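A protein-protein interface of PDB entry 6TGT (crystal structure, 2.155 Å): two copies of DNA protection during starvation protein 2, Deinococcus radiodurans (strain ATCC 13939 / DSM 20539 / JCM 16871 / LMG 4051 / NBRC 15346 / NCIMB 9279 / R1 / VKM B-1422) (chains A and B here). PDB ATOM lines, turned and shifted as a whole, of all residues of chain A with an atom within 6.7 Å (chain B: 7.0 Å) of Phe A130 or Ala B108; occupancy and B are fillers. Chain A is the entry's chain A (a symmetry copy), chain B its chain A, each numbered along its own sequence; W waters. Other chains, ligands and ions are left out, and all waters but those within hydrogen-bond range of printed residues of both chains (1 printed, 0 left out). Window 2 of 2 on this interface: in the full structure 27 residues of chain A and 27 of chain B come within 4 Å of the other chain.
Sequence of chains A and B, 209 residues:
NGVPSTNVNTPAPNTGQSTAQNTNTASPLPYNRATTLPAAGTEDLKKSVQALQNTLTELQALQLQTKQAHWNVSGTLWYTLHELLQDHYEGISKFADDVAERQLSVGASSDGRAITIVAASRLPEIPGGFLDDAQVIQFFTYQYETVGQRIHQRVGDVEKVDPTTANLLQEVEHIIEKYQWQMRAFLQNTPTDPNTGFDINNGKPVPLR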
ATOM      1  N   TRP A  71      28.506 -25.008  22.598  1.00  0.00           N
ATOM      2  CA  TRP A  71      28.263 -25.982  23.655  1.00  0.00           C
ATOM      3  C   TRP A  71      27.253 -25.510  24.691  1.00  0.00           C
ATOM      4  O   TRP A  71      26.505 -26.334  25.231  1.00  0.00           O
ATOM      5  CB  TRP A  71      29.577 -26.337  24.359  1.00  0.00           C
ATOM      6  CG  TRP A  71      30.507 -27.170  23.529  1.00  0.00           C
ATOM      7  CD1 TRP A  71      31.790 -26.862  23.176  1.00  0.00           C
ATOM      8  CD2 TRP A  71      30.229 -28.451  22.948  1.00  0.00           C
ATOM      9  NE1 TRP A  71      32.327 -27.869  22.413  1.00  0.00           N
ATOM     10  CE2 TRP A  71      31.390 -28.857  22.257  1.00  0.00           C
ATOM     11  CE3 TRP A  71      29.113 -29.295  22.944  1.00  0.00           C
ATOM     12  CZ2 TRP A  71      31.464 -30.066  21.570  1.00  0.00           C
ATOM     13  CZ3 TRP A  71      29.190 -30.493  22.261  1.00  0.00           C
ATOM     14  CH2 TRP A  71      30.357 -30.869  21.585  1.00  0.00           C
ATOM     15  N   ASN A  72      27.200 -24.210  24.980  1.00  0.00           N
ATOM     16  CA  ASN A  72      26.397 -23.697  26.083  1.00  0.00           C
ATOM     17  C   ASN A  72      25.153 -22.931  25.651  1.00  0.00           C
ATOM     18  O   ASN A  72      24.471 -22.360  26.509  1.00  0.00           O
ATOM     19  CB  ASN A  72      27.266 -22.811  26.978  1.00  0.00           C
ATOM     20  CG  ASN A  72      28.451 -23.556  27.556  1.00  0.00           C
ATOM     21  OD1 ASN A  72      28.292 -24.439  28.399  1.00  0.00           O
ATOM     22  ND2 ASN A  72      29.648 -23.207  27.102  1.00  0.00           N
ATOM     23  N   VAL A  73      24.828 -22.900  24.357  1.00  0.00           N
ATOM     24  CA  VAL A  73      23.634 -22.176  23.933  1.00  0.00           C
ATOM     25  C   VAL A  73      22.390 -22.899  24.440  1.00  0.00           C
ATOM     26  O   VAL A  73      22.348 -24.134  24.533  1.00  0.00           O
ATOM     27  CB  VAL A  73      23.601 -21.997  22.404  1.00  0.00           C
ATOM     28  CG1 VAL A  73      23.394 -23.330  21.703  1.00  0.00           C
ATOM     29  CG2 VAL A  73      22.525 -20.992  22.001  1.00  0.00           C
ATOM     30  N   SER A  74      21.371 -22.119  24.792  1.00  0.00           N
ATOM     31  CA  SER A  74      20.150 -22.652  25.376  1.00  0.00           C
ATOM     32  C   SER A  74      18.954 -21.897  24.814  1.00  0.00           C
ATOM     33  O   SER A  74      19.082 -20.788  24.289  1.00  0.00           O
ATOM     34  CB  SER A  74      20.165 -22.546  26.906  1.00  0.00           C
ATOM     35  OG  SER A  74      21.342 -23.123  27.446  1.00  0.00           O
ATOM     36  N   PRO A 127      30.212 -14.153  27.239  1.00  0.00           N
ATOM     37  CA  PRO A 127      29.954 -14.481  28.644  1.00  0.00           C
ATOM     38  C   PRO A 127      30.072 -15.972  28.909  1.00  0.00           C
ATOM     39  O   PRO A 127      29.893 -16.807  28.019  1.00  0.00           O
ATOM     40  CB  PRO A 127      28.517 -13.993  28.867  1.00  0.00           C
ATOM     41  CG  PRO A 127      28.285 -12.979  27.800  1.00  0.00           C
ATOM     42  CD  PRO A 127      29.078 -13.444  26.618  1.00  0.00           C
ATOM     43  N   GLY A 128      30.386 -16.301  30.164  1.00  0.00           N
ATOM     44  CA  GLY A 128      30.455 -17.678  30.597  1.00  0.00           C
ATOM     45  C   GLY A 128      29.101 -18.210  31.029  1.00  0.00           C
ATOM     46  O   GLY A 128      28.088 -17.511  31.023  1.00  0.00           O
ATOM     47  N   GLY A 129      29.095 -19.482  31.414  1.00  0.00           N
ATOM     48  CA  GLY A 129      27.864 -20.116  31.833  1.00  0.00           C
ATOM     49  C   GLY A 129      26.933 -20.390  30.662  1.00  0.00           C
ATOM     50  O   GLY A 129      27.286 -20.255  29.490  1.00  0.00           O
ATOM     51  N   PHE A 130      25.712 -20.788  31.011  1.00  0.00           N
ATOM     52  CA  PHE A 130      24.700 -21.075  30.002  1.00  0.00           C
ATOM     53  C   PHE A 130      24.322 -19.801  29.258  1.00  0.00           C
ATOM     54  O   PHE A 130      24.009 -18.776  29.874  1.00  0.00           O
ATOM     55  CB  PHE A 130      23.466 -21.700  30.650  1.00  0.00           C
ATOM     56  CG  PHE A 130      23.707 -23.070  31.214  1.00  0.00           C
ATOM     57  CD1 PHE A 130      23.907 -24.154  30.375  1.00  0.00           C
ATOM     58  CD2 PHE A 130      23.740 -23.274  32.584  1.00  0.00           C
ATOM     59  CE1 PHE A 130      24.131 -25.418  30.892  1.00  0.00           C
ATOM     60  CE2 PHE A 130      23.964 -24.535  33.107  1.00  0.00           C
ATOM     61  CZ  PHE A 130      24.159 -25.608  32.260  1.00  0.00           C
ATOM     62  N   LEU A 131      24.355 -19.865  27.931  1.00  0.00           N
ATOM     63  CA  LEU A 131      24.069 -18.722  27.076  1.00  0.00           C
ATOM     64  C   LEU A 131      22.699 -18.880  26.436  1.00  0.00           C
ATOM     65  O   LEU A 131      22.339 -19.968  25.974  1.00  0.00           O
ATOM     66  CB  LEU A 131      25.134 -18.574  25.988  1.00  0.00           C
ATOM     67  CG  LEU A 131      26.514 -18.100  26.441  1.00  0.00           C
ATOM     68  CD1 LEU A 131      27.484 -18.137  25.275  1.00  0.00           C
ATOM     69  CD2 LEU A 131      26.434 -16.703  27.036  1.00  0.00           C
ATOM     70  N   ASP A 132      21.937 -17.791  26.410  1.00  0.00           N
ATOM     71  CA  ASP A 132      20.636 -17.809  25.763  1.00  0.00           C
ATOM     72  C   ASP A 132      20.791 -17.678  24.253  1.00  0.00           C
ATOM     73  O   ASP A 132      21.750 -17.081  23.754  1.00  0.00           O
ATOM     74  CB  ASP A 132      19.750 -16.682  26.292  1.00  0.00           C
ATOM     75  CG  ASP A 132      18.299 -16.860  25.903  1.00  0.00           C
ATOM     76  OD1 ASP A 132      17.725 -17.919  26.235  1.00  0.00           O
ATOM     77  OD2 ASP A 132      17.732 -15.947  25.266  1.00  0.00           O
ATOM     78  N   GLN A 135      20.753 -14.147  23.172  1.00  0.00           N
ATOM     79  CA  GLN A 135      22.017 -13.510  23.524  1.00  0.00           C
ATOM     80  C   GLN A 135      23.119 -13.896  22.545  1.00  0.00           C
ATOM     81  O   GLN A 135      23.948 -13.057  22.172  1.00  0.00           O
ATOM     82  CB  GLN A 135      22.408 -13.885  24.954  1.00  0.00           C
ATOM     83  CG  GLN A 135      23.623 -13.145  25.489  1.00  0.00           C
ATOM     84  CD  GLN A 135      24.053 -13.653  26.850  1.00  0.00           C
ATOM     85  OE1 GLN A 135      23.645 -14.732  27.279  1.00  0.00           O
ATOM     86  NE2 GLN A 135      24.880 -12.876  27.540  1.00  0.00           N
ATOM     87  N   LEU B  45      28.450 -34.004  41.672  1.00  0.00           N
ATOM     88  CA  LEU B  45      28.570 -33.326  40.387  1.00  0.00           C
ATOM     89  C   LEU B  45      29.800 -32.427  40.352  1.00  0.00           C
ATOM     90  O   LEU B  45      30.435 -32.287  39.301  1.00  0.00           O
ATOM     91  CB  LEU B  45      27.299 -32.516  40.115  1.00  0.00           C
ATOM     92  CG  LEU B  45      27.277 -31.437  39.028  1.00  0.00           C
ATOM     93  CD1 LEU B  45      27.688 -32.011  37.674  1.00  0.00           C
ATOM     94  CD2 LEU B  45      25.902 -30.778  38.955  1.00  0.00           C
ATOM     95  N   VAL B  49      32.828 -32.254  37.355  1.00  0.00           N
ATOM     96  CA  VAL B  49      33.048 -30.981  36.673  1.00  0.00           C
ATOM     97  C   VAL B  49      34.504 -30.556  36.797  1.00  0.00           C
ATOM     98  O   VAL B  49      35.119 -30.100  35.827  1.00  0.00           O
ATOM     99  CB  VAL B  49      32.095 -29.907  37.229  1.00  0.00           C
ATOM    100  CG1 VAL B  49      32.527 -28.520  36.769  1.00  0.00           C
ATOM    101  CG2 VAL B  49      30.671 -30.202  36.804  1.00  0.00           C
ATOM    102  N   ALA B 100      33.909 -31.304  26.678  1.00  0.00           N
ATOM    103  CA  ALA B 100      32.911 -30.265  26.906  1.00  0.00           C
ATOM    104  C   ALA B 100      31.499 -30.801  26.707  1.00  0.00           C
ATOM    105  O   ALA B 100      30.570 -30.394  27.413  1.00  0.00           O
ATOM    106  CB  ALA B 100      33.173 -29.079  25.983  1.00  0.00           C
ATOM    107  N   GLU B 101      31.319 -31.713  25.749  1.00  0.00           N
ATOM    108  CA  GLU B 101      30.020 -32.349  25.567  1.00  0.00           C
ATOM    109  C   GLU B 101      29.635 -33.165  26.794  1.00  0.00           C
ATOM    110  O   GLU B 101      28.469 -33.172  27.206  1.00  0.00           O
ATOM    111  CB  GLU B 101      30.044 -33.231  24.319  1.00  0.00           C
ATOM    112  CG  GLU B 101      28.693 -33.778  23.901  1.00  0.00           C
ATOM    113  CD  GLU B 101      28.775 -34.615  22.638  1.00  0.00           C
ATOM    114  OE1 GLU B 101      29.229 -35.776  22.722  1.00  0.00           O
ATOM    115  OE2 GLU B 101      28.391 -34.110  21.564  1.00  0.00           O
ATOM    116  N   ARG B 102      30.607 -33.860  27.392  1.00  0.00           N
ATOM    117  CA  ARG B 102      30.344 -34.593  28.625  1.00  0.00           C
ATOM    118  C   ARG B 102      30.000 -33.649  29.771  1.00  0.00           C
ATOM    119  O   ARG B 102      29.196 -34.001  30.641  1.00  0.00           O
ATOM    120  CB  ARG B 102      31.555 -35.456  28.983  1.00  0.00           C
ATOM    121  CG  ARG B 102      31.362 -36.342  30.203  1.00  0.00           C
ATOM    122  CD  ARG B 102      30.141 -37.233  30.057  1.00  0.00           C
ATOM    123  NE  ARG B 102      29.953 -38.094  31.220  1.00  0.00           N
ATOM    124  CZ  ARG B 102      28.813 -38.705  31.521  1.00  0.00           C
ATOM    125  NH1 ARG B 102      27.750 -38.551  30.743  1.00  0.00           N
ATOM    126  NH2 ARG B 102      28.733 -39.468  32.602  1.00  0.00           N
ATOM    127  N   GLN B 103      30.592 -32.451  29.784  1.00  0.00           N
ATOM    128  CA  GLN B 103      30.257 -31.460  30.801  1.00  0.00           C
ATOM    129  C   GLN B 103      28.783 -31.087  30.730  1.00  0.00           C
ATOM    130  O   GLN B 103      28.084 -31.071  31.749  1.00  0.00           O
ATOM    131  CB  GLN B 103      31.134 -30.218  30.633  1.00  0.00           C
ATOM    132  CG  GLN B 103      32.490 -30.308  31.304  1.00  0.00           C
ATOM    133  CD  GLN B 103      32.926 -28.988  31.913  1.00  0.00           C
ATOM    134  OE1 GLN B 103      32.439 -28.589  32.971  1.00  0.00           O
ATOM    135  NE2 GLN B 103      33.844 -28.302  31.243  1.00  0.00           N
ATOM    136  N   LEU B 104      28.294 -30.776  29.527  1.00  0.00           N
ATOM    137  CA  LEU B 104      26.880 -30.462  29.365  1.00  0.00           C
ATOM    138  C   LEU B 104      26.003 -31.677  29.635  1.00  0.00           C
ATOM    139  O   LEU B 104      24.865 -31.529  30.094  1.00  0.00           O
ATOM    140  CB  LEU B 104      26.620 -29.924  27.958  1.00  0.00           C
ATOM    141  CG  LEU B 104      26.739 -28.413  27.745  1.00  0.00           C
ATOM    142  CD1 LEU B 104      25.898 -27.654  28.761  1.00  0.00           C
ATOM    143  CD2 LEU B 104      28.193 -27.960  27.798  1.00  0.00           C
ATOM    144  N   SER B 105      26.517 -32.881  29.364  1.00  0.00           N
ATOM    145  CA  SER B 105      25.721 -34.089  29.555  1.00  0.00           C
ATOM    146  C   SER B 105      25.434 -34.339  31.030  1.00  0.00           C
ATOM    147  O   SER B 105      24.345 -34.804  31.385  1.00  0.00           O
ATOM    148  CB  SER B 105      26.434 -35.288  28.933  1.00  0.00           C
ATOM    149  OG  SER B 105      26.607 -35.111  27.539  1.00  0.00           O
ATOM    150  N   VAL B 106      26.400 -34.042  31.908  1.00  0.00           N
ATOM    151  CA  VAL B 106      26.178 -34.194  33.346  1.00  0.00           C
ATOM    152  C   VAL B 106      25.474 -32.995  33.954  1.00  0.00           C
ATOM    153  O   VAL B 106      25.253 -32.974  35.173  1.00  0.00           O
ATOM    154  CB  VAL B 106      27.504 -34.452  34.091  1.00  0.00           C
ATOM    155  CG1 VAL B 106      28.238 -35.635  33.475  1.00  0.00           C
ATOM    156  CG2 VAL B 106      28.378 -33.210  34.083  1.00  0.00           C
ATOM    157  N   GLY B 107      25.116 -32.000  33.152  1.00  0.00           N
ATOM    158  CA  GLY B 107      24.298 -30.896  33.610  1.00  0.00           C
ATOM    159  C   GLY B 107      25.033 -29.647  34.043  1.00  0.00           C
ATOM    160  O   GLY B 107      24.473 -28.867  34.822  1.00  0.00           O
ATOM    161  N   ALA B 108      26.253 -29.421  33.562  1.00  0.00           N
ATOM    162  CA  ALA B 108      27.033 -28.259  33.953  1.00  0.00           C
ATOM    163  C   ALA B 108      27.557 -27.540  32.719  1.00  0.00           C
ATOM    164  O   ALA B 108      27.789 -28.150  31.672  1.00  0.00           O
ATOM    165  CB  ALA B 108      28.202 -28.646  34.857  1.00  0.00           C
ATOM    166  N   SER B 109      27.743 -26.230  32.860  1.00  0.00           N
ATOM    167  CA  SER B 109      28.256 -25.419  31.769  1.00  0.00           C
ATOM    168  C   SER B 109      29.712 -25.762  31.475  1.00  0.00           C
ATOM    169  O   SER B 109      30.428 -26.337  32.300  1.00  0.00           O
ATOM    170  CB  SER B 109      28.134 -23.931  32.101  1.00  0.00           C
ATOM    171  OG  SER B 109      28.117 -23.157  30.916  1.00  0.00           O
ATOM    172  N   SER B 110      30.148 -25.393  30.274  1.00  0.00           N
ATOM    173  CA  SER B 110      31.511 -25.624  29.816  1.00  0.00           C
ATOM    174  C   SER B 110      32.188 -24.285  29.575  1.00  0.00           C
ATOM    175  O   SER B 110      31.637 -23.422  28.884  1.00  0.00           O
ATOM    176  CB  SER B 110      31.526 -26.467  28.538  1.00  0.00           C
ATOM    177  OG  SER B 110      32.852 -26.703  28.106  1.00  0.00           O
HETATM  178  O   HOH W   1      30.820 -21.836  31.311  1.00  0.00           O
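The side-chain hydroxyl (OG) of Ser B109 is in hydrogen-bond range of the side-chain amide oxygen (OD1) of Asn A72 (2.8 Å). The backbone carbonyl oxygen (O) of Gly A129 lies close to the side-chain hydroxyl (OG) of Ser B109, 3.3 Å away. The backbone NH (N) of Phe A130 is in hydrogen-bond range of the side-chain hydroxyl (OG) of Ser B109, 3.4 Å away. ND2 of Asn A72 lies within hydrogen-bond range of O of Ser B110, at 2.7 Å.
The backbone carbonyl oxygen (O) of Glu B101 is in hydrogen-bond range of the side-chain hydroxyl (OG) of Ser B105, 2.7 Å away. O of Gln B103 lies within hydrogen-bond range of N of Ala B108, at 3.1 Å. OE1 of Gln B103 lies close to O of Ser B109. The backbone carbonyl oxygen (O) of Asn A72 lies within hydrogen-bond range of the side-chain hydroxyl (OG) of Ser A74, 3.4 Å away. O of Asn A72 lies within hydrogen-bond range of N of Leu A131.
Among the printed residues, merely in contact across the chains: Trp A71 with Leu B104, Trp A71 with Glu B101, Phe A130 with Leu B104, Asn A72 with Leu B104, Trp A71 with Ala B100 and Phe A130 with Ala B108.
Printed residues of chain B within 4 Å of Phe A130: Leu B104 (3.6 Å), Ala B108 (3.9 Å) and Ser B109 (3.4 Å). Printed residues of chain A within 4 Å of Ala B108: Phe A130. Printed residues of chain B within 4 Å of Gly A129: Ser B109. Of the printed residues of chain A, Ala B100 touches Trp A71. Of the printed residues of chain A, Ser B109 touches Asn A72, Gly A129 and Phe A130. Of the printed residues of chain B, Asn A72 touches Leu B104, Ser B109 and Ser B110. Ser B105 touches none of the printed residues of chain A. The nearest printed residue of chain B that does not touch Trp A71 is Ser B110 (4.6 Å).
Hydrophobic or aromatic side chains of chain B within 4 Å of the printed part of chain A: Ala B100 and Leu B104. Along chain B the printed residues that touch a printed residue of chain A span positions 100 to 110. Of the 11 printed residues of chain A, 4 touch a printed residue of chain B. Among the printed residues, no Asp or Glu carboxylate lies within 4 Å of a Lys or Arg side-chain nitrogen of the other chain.
No position is printed for both chains. Of the 10 pairs that touch across the chains among the printed residues, none has its exchanged pair printed and touching as well.
Water W1 lies within hydrogen-bond range of the backbone NH of Gly A129 (2.9 Å), the backbone carbonyl oxygen of Ser B110 (3.0 Å) and the side-chain hydroxyl of Ser B109 (3.0 Å).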
